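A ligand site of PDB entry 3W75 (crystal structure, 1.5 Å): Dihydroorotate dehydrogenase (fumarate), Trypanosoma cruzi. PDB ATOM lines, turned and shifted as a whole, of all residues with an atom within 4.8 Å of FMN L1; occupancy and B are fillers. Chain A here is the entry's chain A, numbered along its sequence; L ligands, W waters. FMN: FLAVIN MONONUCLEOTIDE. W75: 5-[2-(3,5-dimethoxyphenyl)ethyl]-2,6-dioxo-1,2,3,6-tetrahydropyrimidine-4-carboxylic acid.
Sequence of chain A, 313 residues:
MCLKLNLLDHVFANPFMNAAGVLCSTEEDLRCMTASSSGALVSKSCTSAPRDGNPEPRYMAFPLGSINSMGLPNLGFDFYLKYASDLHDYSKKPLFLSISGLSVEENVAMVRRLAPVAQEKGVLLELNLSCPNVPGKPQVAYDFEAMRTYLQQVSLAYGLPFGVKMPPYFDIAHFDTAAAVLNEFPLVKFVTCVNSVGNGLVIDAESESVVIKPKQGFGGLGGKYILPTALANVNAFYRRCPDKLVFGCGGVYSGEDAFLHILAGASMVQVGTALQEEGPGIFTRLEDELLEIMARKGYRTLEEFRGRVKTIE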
ATOM      1  N   ALA A  19      25.362  -3.325  29.308  1.00  0.00           N
ATOM      2  CA  ALA A  19      24.774  -4.370  28.473  1.00  0.00           C
ATOM      3  C   ALA A  19      25.756  -5.519  28.387  1.00  0.00           C
ATOM      4  O   ALA A  19      26.993  -5.345  28.321  1.00  0.00           O
ATOM      5  CB  ALA A  19      24.523  -3.846  27.082  1.00  0.00           C
ATOM      6  N   ALA A  20      25.238  -6.766  28.352  1.00  0.00           N
ATOM      7  CA  ALA A  20      26.097  -7.915  28.275  1.00  0.00           C
ATOM      8  C   ALA A  20      26.988  -7.757  27.048  1.00  0.00           C
ATOM      9  O   ALA A  20      26.577  -7.297  25.973  1.00  0.00           O
ATOM     10  CB  ALA A  20      25.305  -9.203  28.252  1.00  0.00           C
ATOM     11  N   GLY A  21      28.238  -8.173  27.232  1.00  0.00           N
ATOM     12  CA  GLY A  21      29.240  -8.087  26.227  1.00  0.00           C
ATOM     13  C   GLY A  21      30.118  -6.913  26.187  1.00  0.00           C
ATOM     14  O   GLY A  21      31.194  -6.928  25.642  1.00  0.00           O
ATOM     15  N   VAL A  22      29.626  -5.792  26.784  1.00  0.00           N
ATOM     16  CA  VAL A  22      30.399  -4.563  26.835  1.00  0.00           C
ATOM     17  C   VAL A  22      31.047  -4.398  28.216  1.00  0.00           C
ATOM     18  O   VAL A  22      30.352  -4.460  29.252  1.00  0.00           O
ATOM     19  CB  VAL A  22      29.509  -3.326  26.518  1.00  0.00           C
ATOM     20  CG1 VAL A  22      30.262  -2.049  26.667  1.00  0.00           C
ATOM     21  CG2 VAL A  22      28.930  -3.534  25.142  1.00  0.00           C
ATOM     22  N   LYS A  44      29.995 -11.022  30.375  1.00  0.00           N
ATOM     23  CA  LYS A  44      29.946 -11.383  28.962  1.00  0.00           C
ATOM     24  C   LYS A  44      29.203 -12.700  28.854  1.00  0.00           C
ATOM     25  O   LYS A  44      29.441 -13.618  29.650  1.00  0.00           O
ATOM     26  CB  LYS A  44      31.367 -11.614  28.491  1.00  0.00           C
ATOM     27  CG  LYS A  44      31.464 -12.220  27.142  1.00  0.00           C
ATOM     28  CD  LYS A  44      30.997 -11.332  25.942  1.00  0.00           C
ATOM     29  CE  LYS A  44      30.821 -12.024  24.606  1.00  0.00           C
ATOM     30  NZ  LYS A  44      30.221 -11.189  23.503  1.00  0.00           N
ATOM     31  N   SER A  45      28.380 -12.902  27.847  1.00  0.00           N
ATOM     32  CA  SER A  45      27.748 -14.211  27.670  1.00  0.00           C
ATOM     33  C   SER A  45      28.803 -15.269  27.491  1.00  0.00           C
ATOM     34  O   SER A  45      29.761 -15.108  26.723  1.00  0.00           O
ATOM     35  CB  SER A  45      26.854 -14.205  26.445  1.00  0.00           C
ATOM     36  OG  SER A  45      25.704 -13.357  26.603  1.00  0.00           O
ATOM     37  N   TYR A  59      34.241  -5.251  15.640  1.00  0.00           N
ATOM     38  CA  TYR A  59      33.390  -4.187  16.251  1.00  0.00           C
ATOM     39  C   TYR A  59      33.783  -2.872  15.620  1.00  0.00           C
ATOM     40  O   TYR A  59      35.000  -2.578  15.542  1.00  0.00           O
ATOM     41  CB  TYR A  59      33.545  -4.109  17.734  1.00  0.00           C
ATOM     42  CG  TYR A  59      32.863  -2.891  18.352  1.00  0.00           C
ATOM     43  CD1 TYR A  59      31.517  -2.854  18.710  1.00  0.00           C
ATOM     44  CD2 TYR A  59      33.573  -1.741  18.567  1.00  0.00           C
ATOM     45  CE1 TYR A  59      30.930  -1.755  19.277  1.00  0.00           C
ATOM     46  CE2 TYR A  59      32.968  -0.610  19.122  1.00  0.00           C
ATOM     47  CZ  TYR A  59      31.677  -0.629  19.445  1.00  0.00           C
ATOM     48  OH  TYR A  59      31.055   0.442  20.009  1.00  0.00           O
ATOM     49  N   SER A  66      26.715   1.283  16.371  1.00  0.00           N
ATOM     50  CA  SER A  66      27.786   0.338  16.224  1.00  0.00           C
ATOM     51  C   SER A  66      27.318  -0.886  15.461  1.00  0.00           C
ATOM     52  O   SER A  66      26.111  -1.189  15.389  1.00  0.00           O
ATOM     53  CB  SER A  66      28.332  -0.109  17.564  1.00  0.00           C
ATOM     54  OG  SER A  66      27.388  -0.868  18.302  1.00  0.00           O
ATOM     55  N   ASN A  68      28.642  -5.179  15.220  1.00  0.00           N
ATOM     56  CA  ASN A  68      29.553  -6.196  15.791  1.00  0.00           C
ATOM     57  C   ASN A  68      29.201  -7.541  15.300  1.00  0.00           C
ATOM     58  O   ASN A  68      28.082  -7.958  15.157  1.00  0.00           O
ATOM     59  CB  ASN A  68      29.604  -6.148  17.294  1.00  0.00           C
ATOM     60  CG  ASN A  68      28.553  -6.987  17.950  1.00  0.00           C
ATOM     61  OD1 ASN A  68      28.700  -8.209  18.143  1.00  0.00           O
ATOM     62  ND2 ASN A  68      27.472  -6.369  18.356  1.00  0.00           N
ATOM     63  N   MET A  70      31.199 -10.204  17.101  1.00  0.00           N
ATOM     64  CA  MET A  70      32.255 -10.643  18.010  1.00  0.00           C
ATOM     65  C   MET A  70      32.457 -12.140  17.916  1.00  0.00           C
ATOM     66  O   MET A  70      33.665 -12.544  18.025  1.00  0.00           O
ATOM     67  CB  MET A  70      32.003 -10.212  19.443  1.00  0.00           C
ATOM     68  CG  MET A  70      31.710  -8.736  19.689  1.00  0.00           C
ATOM     69  SD  MET A  70      32.999  -7.670  19.137  1.00  0.00           S
ATOM     70  CE  MET A  70      34.144  -7.976  20.326  1.00  0.00           C
ATOM     71  N   LEU A  72      31.031 -14.405  20.189  1.00  0.00           N
ATOM     72  CA  LEU A  72      30.949 -14.916  21.536  1.00  0.00           C
ATOM     73  C   LEU A  72      32.309 -15.181  22.094  1.00  0.00           C
ATOM     74  O   LEU A  72      32.521 -16.256  22.755  1.00  0.00           O
ATOM     75  CB  LEU A  72      30.006 -16.124  21.509  1.00  0.00           C
ATOM     76  CG  LEU A  72      29.384 -16.743  22.671  1.00  0.00           C
ATOM     77  CD1 LEU A  72      28.777 -15.697  23.628  1.00  0.00           C
ATOM     78  CD2 LEU A  72      28.311 -17.705  22.200  1.00  0.00           C
ATOM     79  N   SER A  98      25.548 -13.788  32.435  1.00  0.00           N
ATOM     80  CA  SER A  98      24.904 -14.091  31.154  1.00  0.00           C
ATOM     81  C   SER A  98      25.442 -15.367  30.592  1.00  0.00           C
ATOM     82  O   SER A  98      26.670 -15.596  30.533  1.00  0.00           O
ATOM     83  CB  SER A  98      25.121 -12.962  30.103  1.00  0.00           C
ATOM     84  OG  SER A  98      24.526 -13.358  28.897  1.00  0.00           O
ATOM     85  N   GLU A 126      21.007 -14.230  33.558  1.00  0.00           N
ATOM     86  CA  GLU A 126      20.402 -13.772  32.312  1.00  0.00           C
ATOM     87  C   GLU A 126      20.739 -14.786  31.208  1.00  0.00           C
ATOM     88  O   GLU A 126      21.832 -14.939  30.854  1.00  0.00           O
ATOM     89  CB  GLU A 126      20.875 -12.311  32.002  1.00  0.00           C
ATOM     90  CG  GLU A 126      20.213 -11.595  30.751  1.00  0.00           C
ATOM     91  CD  GLU A 126      20.721 -10.138  30.414  1.00  0.00           C
ATOM     92  OE1 GLU A 126      21.746  -9.993  29.783  1.00  0.00           O
ATOM     93  OE2 GLU A 126      20.087  -9.138  30.755  1.00  0.00           O
ATOM     94  N   ASN A 128      20.857 -15.742  27.559  1.00  0.00           N
ATOM     95  CA  ASN A 128      20.926 -15.137  26.221  1.00  0.00           C
ATOM     96  C   ASN A 128      20.456 -16.092  25.166  1.00  0.00           C
ATOM     97  O   ASN A 128      21.185 -17.062  24.895  1.00  0.00           O
ATOM     98  CB  ASN A 128      22.332 -14.621  25.931  1.00  0.00           C
ATOM     99  CG  ASN A 128      22.501 -13.972  24.572  1.00  0.00           C
ATOM    100  OD1 ASN A 128      21.535 -13.749  23.863  1.00  0.00           O
ATOM    101  ND2 ASN A 128      23.735 -13.673  24.234  1.00  0.00           N
ATOM    102  N   LYS A 165      17.378 -12.687  27.802  1.00  0.00           N
ATOM    103  CA  LYS A 165      17.781 -11.637  26.850  1.00  0.00           C
ATOM    104  C   LYS A 165      17.222 -12.018  25.466  1.00  0.00           C
ATOM    105  O   LYS A 165      17.534 -13.038  24.922  1.00  0.00           O
ATOM    106  CB  LYS A 165      19.246 -11.459  26.846  1.00  0.00           C
ATOM    107  CG  LYS A 165      19.851 -10.465  25.824  1.00  0.00           C
ATOM    108  CD  LYS A 165      19.751  -9.125  26.390  1.00  0.00           C
ATOM    109  CE  LYS A 165      20.468  -8.069  25.530  1.00  0.00           C
ATOM    110  NZ  LYS A 165      21.936  -8.079  25.737  1.00  0.00           N
ATOM    111  N   VAL A 194      16.508  -4.897  24.257  1.00  0.00           N
ATOM    112  CA  VAL A 194      16.746  -5.914  23.243  1.00  0.00           C
ATOM    113  C   VAL A 194      18.259  -6.147  23.073  1.00  0.00           C
ATOM    114  O   VAL A 194      19.102  -5.260  23.391  1.00  0.00           O
ATOM    115  CB  VAL A 194      16.172  -5.486  21.871  1.00  0.00           C
ATOM    116  CG1 VAL A 194      14.644  -5.505  21.919  1.00  0.00           C
ATOM    117  CG2 VAL A 194      16.736  -4.157  21.378  1.00  0.00           C
ATOM    118  N   ASN A 195      18.577  -7.345  22.539  1.00  0.00           N
ATOM    119  CA  ASN A 195      19.862  -7.572  21.903  1.00  0.00           C
ATOM    120  C   ASN A 195      19.992  -6.692  20.672  1.00  0.00           C
ATOM    121  O   ASN A 195      19.066  -5.961  20.250  1.00  0.00           O
ATOM    122  CB  ASN A 195      20.017  -9.071  21.603  1.00  0.00           C
ATOM    123  CG  ASN A 195      21.432  -9.530  21.814  1.00  0.00           C
ATOM    124  OD1 ASN A 195      22.370  -8.932  21.276  1.00  0.00           O
ATOM    125  ND2 ASN A 195      21.568 -10.680  22.447  1.00  0.00           N
ATOM    126  N   SER A 196      21.162  -6.703  20.086  1.00  0.00           N
ATOM    127  CA  SER A 196      21.408  -5.908  18.856  1.00  0.00           C
ATOM    128  C   SER A 196      20.463  -6.347  17.745  1.00  0.00           C
ATOM    129  O   SER A 196      19.921  -7.475  17.738  1.00  0.00           O
ATOM    130  CB  SER A 196      22.887  -6.017  18.491  1.00  0.00           C
ATOM    131  OG  SER A 196      23.239  -7.357  18.282  1.00  0.00           O
ATOM    132  N   GLY A 222      23.788  -1.720  17.165  1.00  0.00           N
ATOM    133  CA  GLY A 222      23.446  -1.095  18.399  1.00  0.00           C
ATOM    134  C   GLY A 222      23.495   0.419  18.267  1.00  0.00           C
ATOM    135  O   GLY A 222      23.940   0.970  17.238  1.00  0.00           O
ATOM    136  N   GLY A 223      23.094   1.100  19.354  1.00  0.00           N
ATOM    137  CA  GLY A 223      23.156   2.534  19.395  1.00  0.00           C
ATOM    138  C   GLY A 223      21.934   3.304  18.912  1.00  0.00           C
ATOM    139  O   GLY A 223      20.811   2.833  19.000  1.00  0.00           O
ATOM    140  N   ILE A 226      18.831   2.002  16.910  1.00  0.00           N
ATOM    141  CA  ILE A 226      17.919   1.051  17.429  1.00  0.00           C
ATOM    142  C   ILE A 226      17.025   1.484  18.537  1.00  0.00           C
ATOM    143  O   ILE A 226      16.191   0.710  18.994  1.00  0.00           O
ATOM    144  CB  ILE A 226      18.621  -0.299  17.778  1.00  0.00           C
ATOM    145  CG1 ILE A 226      19.317  -0.267  19.174  1.00  0.00           C
ATOM    146  CG2 ILE A 226      19.576  -0.739  16.696  1.00  0.00           C
ATOM    147  CD1 ILE A 226      19.656  -1.647  19.697  1.00  0.00           C
ATOM    148  N   CYS A 249      17.247  -2.217  26.961  1.00  0.00           N
ATOM    149  CA  CYS A 249      18.538  -2.109  26.377  1.00  0.00           C
ATOM    150  C   CYS A 249      18.372  -1.690  24.985  1.00  0.00           C
ATOM    151  O   CYS A 249      17.620  -2.265  24.195  1.00  0.00           O
ATOM    152  CB  CYS A 249      19.216  -3.487  26.391  1.00  0.00           C
ATOM    153  SG  CYS A 249      20.980  -3.439  26.005  1.00  0.00           S
ATOM    154  N   GLY A 250      19.118  -0.668  24.560  1.00  0.00           N
ATOM    155  CA  GLY A 250      19.191  -0.259  23.161  1.00  0.00           C
ATOM    156  C   GLY A 250      19.128   1.228  23.038  1.00  0.00           C
ATOM    157  O   GLY A 250      18.132   1.854  23.392  1.00  0.00           O
ATOM    158  N   GLY A 251      20.171   1.821  22.531  1.00  0.00           N
ATOM    159  CA  GLY A 251      20.139   3.207  22.180  1.00  0.00           C
ATOM    160  C   GLY A 251      20.254   4.169  23.279  1.00  0.00           C
ATOM    161  O   GLY A 251      19.918   5.366  23.098  1.00  0.00           O
ATOM    162  N   VAL A 252      20.686   3.781  24.477  1.00  0.00           N
ATOM    163  CA  VAL A 252      20.778   4.720  25.584  1.00  0.00           C
ATOM    164  C   VAL A 252      22.113   5.457  25.489  1.00  0.00           C
ATOM    165  O   VAL A 252      23.180   4.861  25.664  1.00  0.00           O
ATOM    166  CB  VAL A 252      20.632   4.041  26.904  1.00  0.00           C
ATOM    167  CG1 VAL A 252      20.865   5.011  28.076  1.00  0.00           C
ATOM    168  CG2 VAL A 252      19.256   3.388  27.026  1.00  0.00           C
ATOM    169  N   GLN A 270      20.036  -0.827  30.531  1.00  0.00           N
ATOM    170  CA  GLN A 270      21.362  -1.316  30.159  1.00  0.00           C
ATOM    171  C   GLN A 270      21.959  -0.434  29.036  1.00  0.00           C
ATOM    172  O   GLN A 270      21.227   0.128  28.210  1.00  0.00           O
ATOM    173  CB  GLN A 270      21.366  -2.694  29.714  1.00  0.00           C
ATOM    174  CG  GLN A 270      20.518  -3.670  30.602  1.00  0.00           C
ATOM    175  CD  GLN A 270      20.687  -5.083  30.223  1.00  0.00           C
ATOM    176  OE1 GLN A 270      20.967  -5.428  29.024  1.00  0.00           O
ATOM    177  NE2 GLN A 270      20.574  -5.968  31.154  1.00  0.00           N
ATOM    178  N   VAL A 271      23.280  -0.270  29.078  1.00  0.00           N
ATOM    179  CA  VAL A 271      24.002   0.621  28.178  1.00  0.00           C
ATOM    180  C   VAL A 271      25.145  -0.166  27.486  1.00  0.00           C
ATOM    181  O   VAL A 271      26.006  -0.692  28.174  1.00  0.00           O
ATOM    182  CB  VAL A 271      24.591   1.786  29.013  1.00  0.00           C
ATOM    183  CG1 VAL A 271      25.145   2.779  28.056  1.00  0.00           C
ATOM    184  CG2 VAL A 271      23.505   2.405  29.911  1.00  0.00           C
ATOM    185  N   GLY A 272      25.069  -0.308  26.141  1.00  0.00           N
ATOM    186  CA  GLY A 272      25.985  -1.008  25.347  1.00  0.00           C
ATOM    187  C   GLY A 272      26.914  -0.119  24.578  1.00  0.00           C
ATOM    188  O   GLY A 272      27.989   0.288  25.119  1.00  0.00           O
ATOM    189  N   THR A 273      26.564   0.178  23.358  1.00  0.00           N
ATOM    190  CA  THR A 273      27.402   1.046  22.519  1.00  0.00           C
ATOM    191  C   THR A 273      27.879   2.292  23.183  1.00  0.00           C
ATOM    192  O   THR A 273      29.059   2.617  23.061  1.00  0.00           O
ATOM    193  CB  THR A 273      26.571   1.367  21.241  1.00  0.00           C
ATOM    194  OG1 THR A 273      26.230   0.169  20.540  1.00  0.00           O
ATOM    195  CG2 THR A 273      27.394   2.234  20.320  1.00  0.00           C
ATOM    196  N   ALA A 274      26.982   3.024  23.819  1.00  0.00           N
ATOM    197  CA  ALA A 274      27.448   4.279  24.421  1.00  0.00           C
ATOM    198  C   ALA A 274      28.479   4.063  25.509  1.00  0.00           C
ATOM    199  O   ALA A 274      29.357   4.919  25.669  1.00  0.00           O
ATOM    200  CB  ALA A 274      26.243   5.059  24.926  1.00  0.00           C
HETATM  201  N1  FMN L   1      24.500  -9.165  24.152  1.00  0.00           N
HETATM  202  C2  FMN L   1      24.466 -10.275  24.899  1.00  0.00           C
HETATM  203  O2  FMN L   1      23.410 -10.591  25.486  1.00  0.00           O
HETATM  204  N3  FMN L   1      25.614 -11.011  25.173  1.00  0.00           N
HETATM  205  C4  FMN L   1      26.735 -10.662  24.643  1.00  0.00           C
HETATM  206  O4  FMN L   1      27.798 -11.316  24.929  1.00  0.00           O
HETATM  207  C4A FMN L   1      26.859  -9.513  23.834  1.00  0.00           C
HETATM  208  N5  FMN L   1      28.041  -9.090  23.260  1.00  0.00           N
HETATM  209  C5A FMN L   1      28.091  -7.823  22.746  1.00  0.00           C
HETATM  210  C6  FMN L   1      29.289  -7.328  22.345  1.00  0.00           C
HETATM  211  C7  FMN L   1      29.379  -6.054  21.794  1.00  0.00           C
HETATM  212  C7M FMN L   1      30.766  -5.481  21.412  1.00  0.00           C
HETATM  213  C8  FMN L   1      28.240  -5.259  21.592  1.00  0.00           C
HETATM  214  C8M FMN L   1      28.329  -3.905  20.981  1.00  0.00           C
HETATM  215  C9  FMN L   1      27.046  -5.799  21.973  1.00  0.00           C
HETATM  216  C9A FMN L   1      26.922  -7.046  22.540  1.00  0.00           C
HETATM  217  N10 FMN L   1      25.698  -7.551  22.939  1.00  0.00           N
HETATM  218  C10 FMN L   1      25.643  -8.738  23.644  1.00  0.00           C
HETATM  219  C1' FMN L   1      24.449  -6.827  22.736  1.00  0.00           C
HETATM  220  C2' FMN L   1      24.308  -5.735  23.790  1.00  0.00           C
HETATM  221  O2' FMN L   1      24.165  -6.338  25.090  1.00  0.00           O
HETATM  222  C3' FMN L   1      23.085  -4.844  23.539  1.00  0.00           C
HETATM  223  O3' FMN L   1      21.918  -5.723  23.621  1.00  0.00           O
HETATM  224  C4' FMN L   1      23.080  -4.138  22.194  1.00  0.00           C
HETATM  225  O4' FMN L   1      24.425  -3.669  21.857  1.00  0.00           O
HETATM  226  C5' FMN L   1      22.124  -2.948  22.101  1.00  0.00           C
HETATM  227  O5' FMN L   1      22.349  -2.022  23.141  1.00  0.00           O
HETATM  228  P   FMN L   1      23.067  -0.612  22.694  1.00  0.00           P
HETATM  229  O1P FMN L   1      23.200   0.113  23.965  1.00  0.00           O
HETATM  230  O2P FMN L   1      22.187   0.070  21.703  1.00  0.00           O
HETATM  231  O3P FMN L   1      24.417  -0.980  22.094  1.00  0.00           O
HETATM  232  OAJ W75 L   2      29.462 -12.088  20.822  1.00  0.00           O
HETATM  233  CAI W75 L   2      28.696 -11.510  19.973  1.00  0.00           C
HETATM  234  OAK W75 L   2      28.936 -11.351  18.741  1.00  0.00           O
HETATM  235  C4  W75 L   2      27.345 -11.088  20.392  1.00  0.00           C
HETATM  236  N3  W75 L   2      26.980  -9.816  19.856  1.00  0.00           N
HETATM  237  C2  W75 L   2      25.748  -9.297  20.086  1.00  0.00           C
HETATM  238  O2  W75 L   2      25.464  -8.143  19.628  1.00  0.00           O
HETATM  239  N1  W75 L   2      24.879  -9.982  20.861  1.00  0.00           N
HETATM  240  C6  W75 L   2      25.180 -11.225  21.401  1.00  0.00           C
HETATM  241  O6  W75 L   2      24.274 -11.778  22.052  1.00  0.00           O
HETATM  242  C5  W75 L   2      26.463 -11.778  21.166  1.00  0.00           C
HETATM  243  CAL W75 L   2      26.764 -13.164  21.705  1.00  0.00           C
HETATM  244  CAM W75 L   2      25.907 -14.235  21.003  1.00  0.00           C
HETATM  245  CAN W75 L   2      26.035 -14.192  19.579  1.00  0.00           C
HETATM  246  CAS W75 L   2      27.227 -14.140  18.844  1.00  0.00           C
HETATM  247  CAO W75 L   2      24.927 -14.018  18.735  1.00  0.00           C
HETATM  248  CAP W75 L   2      24.980 -13.955  17.374  1.00  0.00           C
HETATM  249  OAU W75 L   2      23.728 -13.759  16.746  1.00  0.00           O
HETATM  250  CAW W75 L   2      23.805 -13.873  15.427  1.00  0.00           C
HETATM  251  CAQ W75 L   2      26.157 -13.899  16.697  1.00  0.00           C
HETATM  252  CAR W75 L   2      27.312 -14.035  17.466  1.00  0.00           C
HETATM  253  OAT W75 L   2      28.579 -13.994  16.920  1.00  0.00           O
HETATM  254  CAV W75 L   2      28.676 -13.500  15.574  1.00  0.00           C
HETATM  255  O   HOH W   1      32.107  -8.962  23.567  1.00  0.00           O
HETATM  256  O   HOH W   2      21.213   0.989  25.558  1.00  0.00           O
HETATM  257  O   HOH W   3      22.714 -11.735  27.956  1.00  0.00           O
HETATM  258  O   HOH W   4      24.182   2.647  23.970  1.00  0.00           O
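The backbone NH (N) of Thr 273 sits at hydrogen-bond distance from an oxygen (O3P) of FMN L1 (2.7 Å).
OG1 of Thr 273 sits at hydrogen-bond distance from O3P of FMN L1.
O2P of FMN L1 lies within hydrogen-bond range of N of Gly 223 (2.7 Å).
The backbone NH of Ala 20 sits at hydrogen-bond distance from an oxygen (O2') of FMN L1, at 3.5 Å.
O2' of FMN L1 lies within hydrogen-bond range of O of Ala 20 (2.7 Å).
O4 of FMN L1 is in hydrogen-bond range of N of Ser 45, 3.4 Å away.
The side-chain hydroxyl (OG) of Ser 45 sits at hydrogen-bond distance from a nitrogen (N3) of FMN L1 (2.7 Å).
O2P of FMN L1 is in hydrogen-bond range of N of Gly 251 (2.8 Å).
NZ of Lys 44 lies within hydrogen-bond range of O4 of FMN L1 (2.8 Å).
O3' of FMN L1 lies within hydrogen-bond range of O of Val 194.
N of Gly 272 sits at hydrogen-bond distance from O1P of FMN L1 (2.9 Å).
The side-chain amino group of Lys 165 sits at hydrogen-bond distance from an oxygen (O2') of FMN L1 (2.9 Å).
An oxygen (O2) of FMN L1 is in hydrogen-bond range of the side-chain amide nitrogen (ND2) of Asn 128 (3.3 Å).
The side-chain sulfur of Cys 249 lies within hydrogen-bond range of an oxygen (O3') of FMN L1.
The side-chain amino group of Lys 44 is in salt-bridge range of an oxygen (OAJ) of W75 L2.
N1 of W75 L2 sits at hydrogen-bond distance from OD1 of Asn 195 (2.8 Å).
ND2 of Asn 128 is in hydrogen-bond range of O6 of W75 L2 (2.9 Å).
OD1 of Asn 68 is in hydrogen-bond range of N3 of W75 L2, at 2.9 Å.
OG of Ser 196 lies within hydrogen-bond range of O2 of W75 L2 (2.7 Å).
The backbone NH of Met 70 sits at hydrogen-bond distance from an oxygen (OAK) of W75 L2, at 3.0 Å.
OAJ of W75 L2 sits at hydrogen-bond distance from N of Leu 72 (2.9 Å).
N1 of W75 L2 lies close to N1 of FMN L1.
N of Gly 223 lies within hydrogen-bond range of OG1 of Thr 273 (3.5 Å).
OG1 of Thr 273 sits at hydrogen-bond distance from OG of Ser 66 (2.7 Å).
The side-chain hydroxyl of Ser 45 sits at hydrogen-bond distance from the side-chain hydroxyl of Ser 98, 2.6 Å away.
O of Cys 249 sits at hydrogen-bond distance from N of Val 194 (2.9 Å).
The side-chain amide nitrogen (ND2) of Asn 195 lies within hydrogen-bond range of the side-chain amide oxygen (OD1) of Asn 128 (3.4 Å).
OD1 of Asn 195 is in hydrogen-bond range of OG of Ser 196 (3.5 Å).
The side-chain amide oxygen (OD1) of Asn 68 lies within hydrogen-bond range of the backbone NH (N) of Met 70, at 3.4 Å.
The backbone NH of Ser 66 lies within hydrogen-bond range of the backbone carbonyl oxygen of Gly 222.
CB of Ala 19 touches O2' of FMN L1 (3.2 Å).
Gly 21 touches FMN L1.
CE1 of Tyr 59 touches C8M of FMN L1, at 3.8 Å.
Asn 68 touches FMN L1.
Met 70 touches FMN L1.
Asn 195 touches FMN L1 (CA to O3', 3.3 Å).
N of Ser 196 touches O3' of FMN L1 (3.7 Å).
Gly 222 touches FMN L1 (C to O2P, 3.7 Å).
CD1 of Ile 226 touches O2P of FMN L1, 3.7 Å away.
Gly 250 touches FMN L1 (CA to O2P, 3.3 Å).
Hydrophobic or aromatic side chains within 4 Å of FMN L1: Ala 19, Ala 20, Tyr 59, Met 70 and Ile 226.
Of the 30 residues printed, 21 come within 4 Å of FMN L1.
The nearest printed residue that does not touch FMN L1 is Val 22 (4.01 Å).
Water W4 lies within hydrogen-bond range of an oxygen (O1P) of FMN L1, the backbone NH of Ala 274, the backbone carbonyl oxygen of Val 252 and the backbone NH of Thr 273.
Water W3 lies within hydrogen-bond range of OG of Ser 98, OE1 of Glu 126 and O2 of FMN L1.
Water W1 bridges NZ of Lys 44 (2.9 Å) and O of Gly 21 (3.0 Å).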
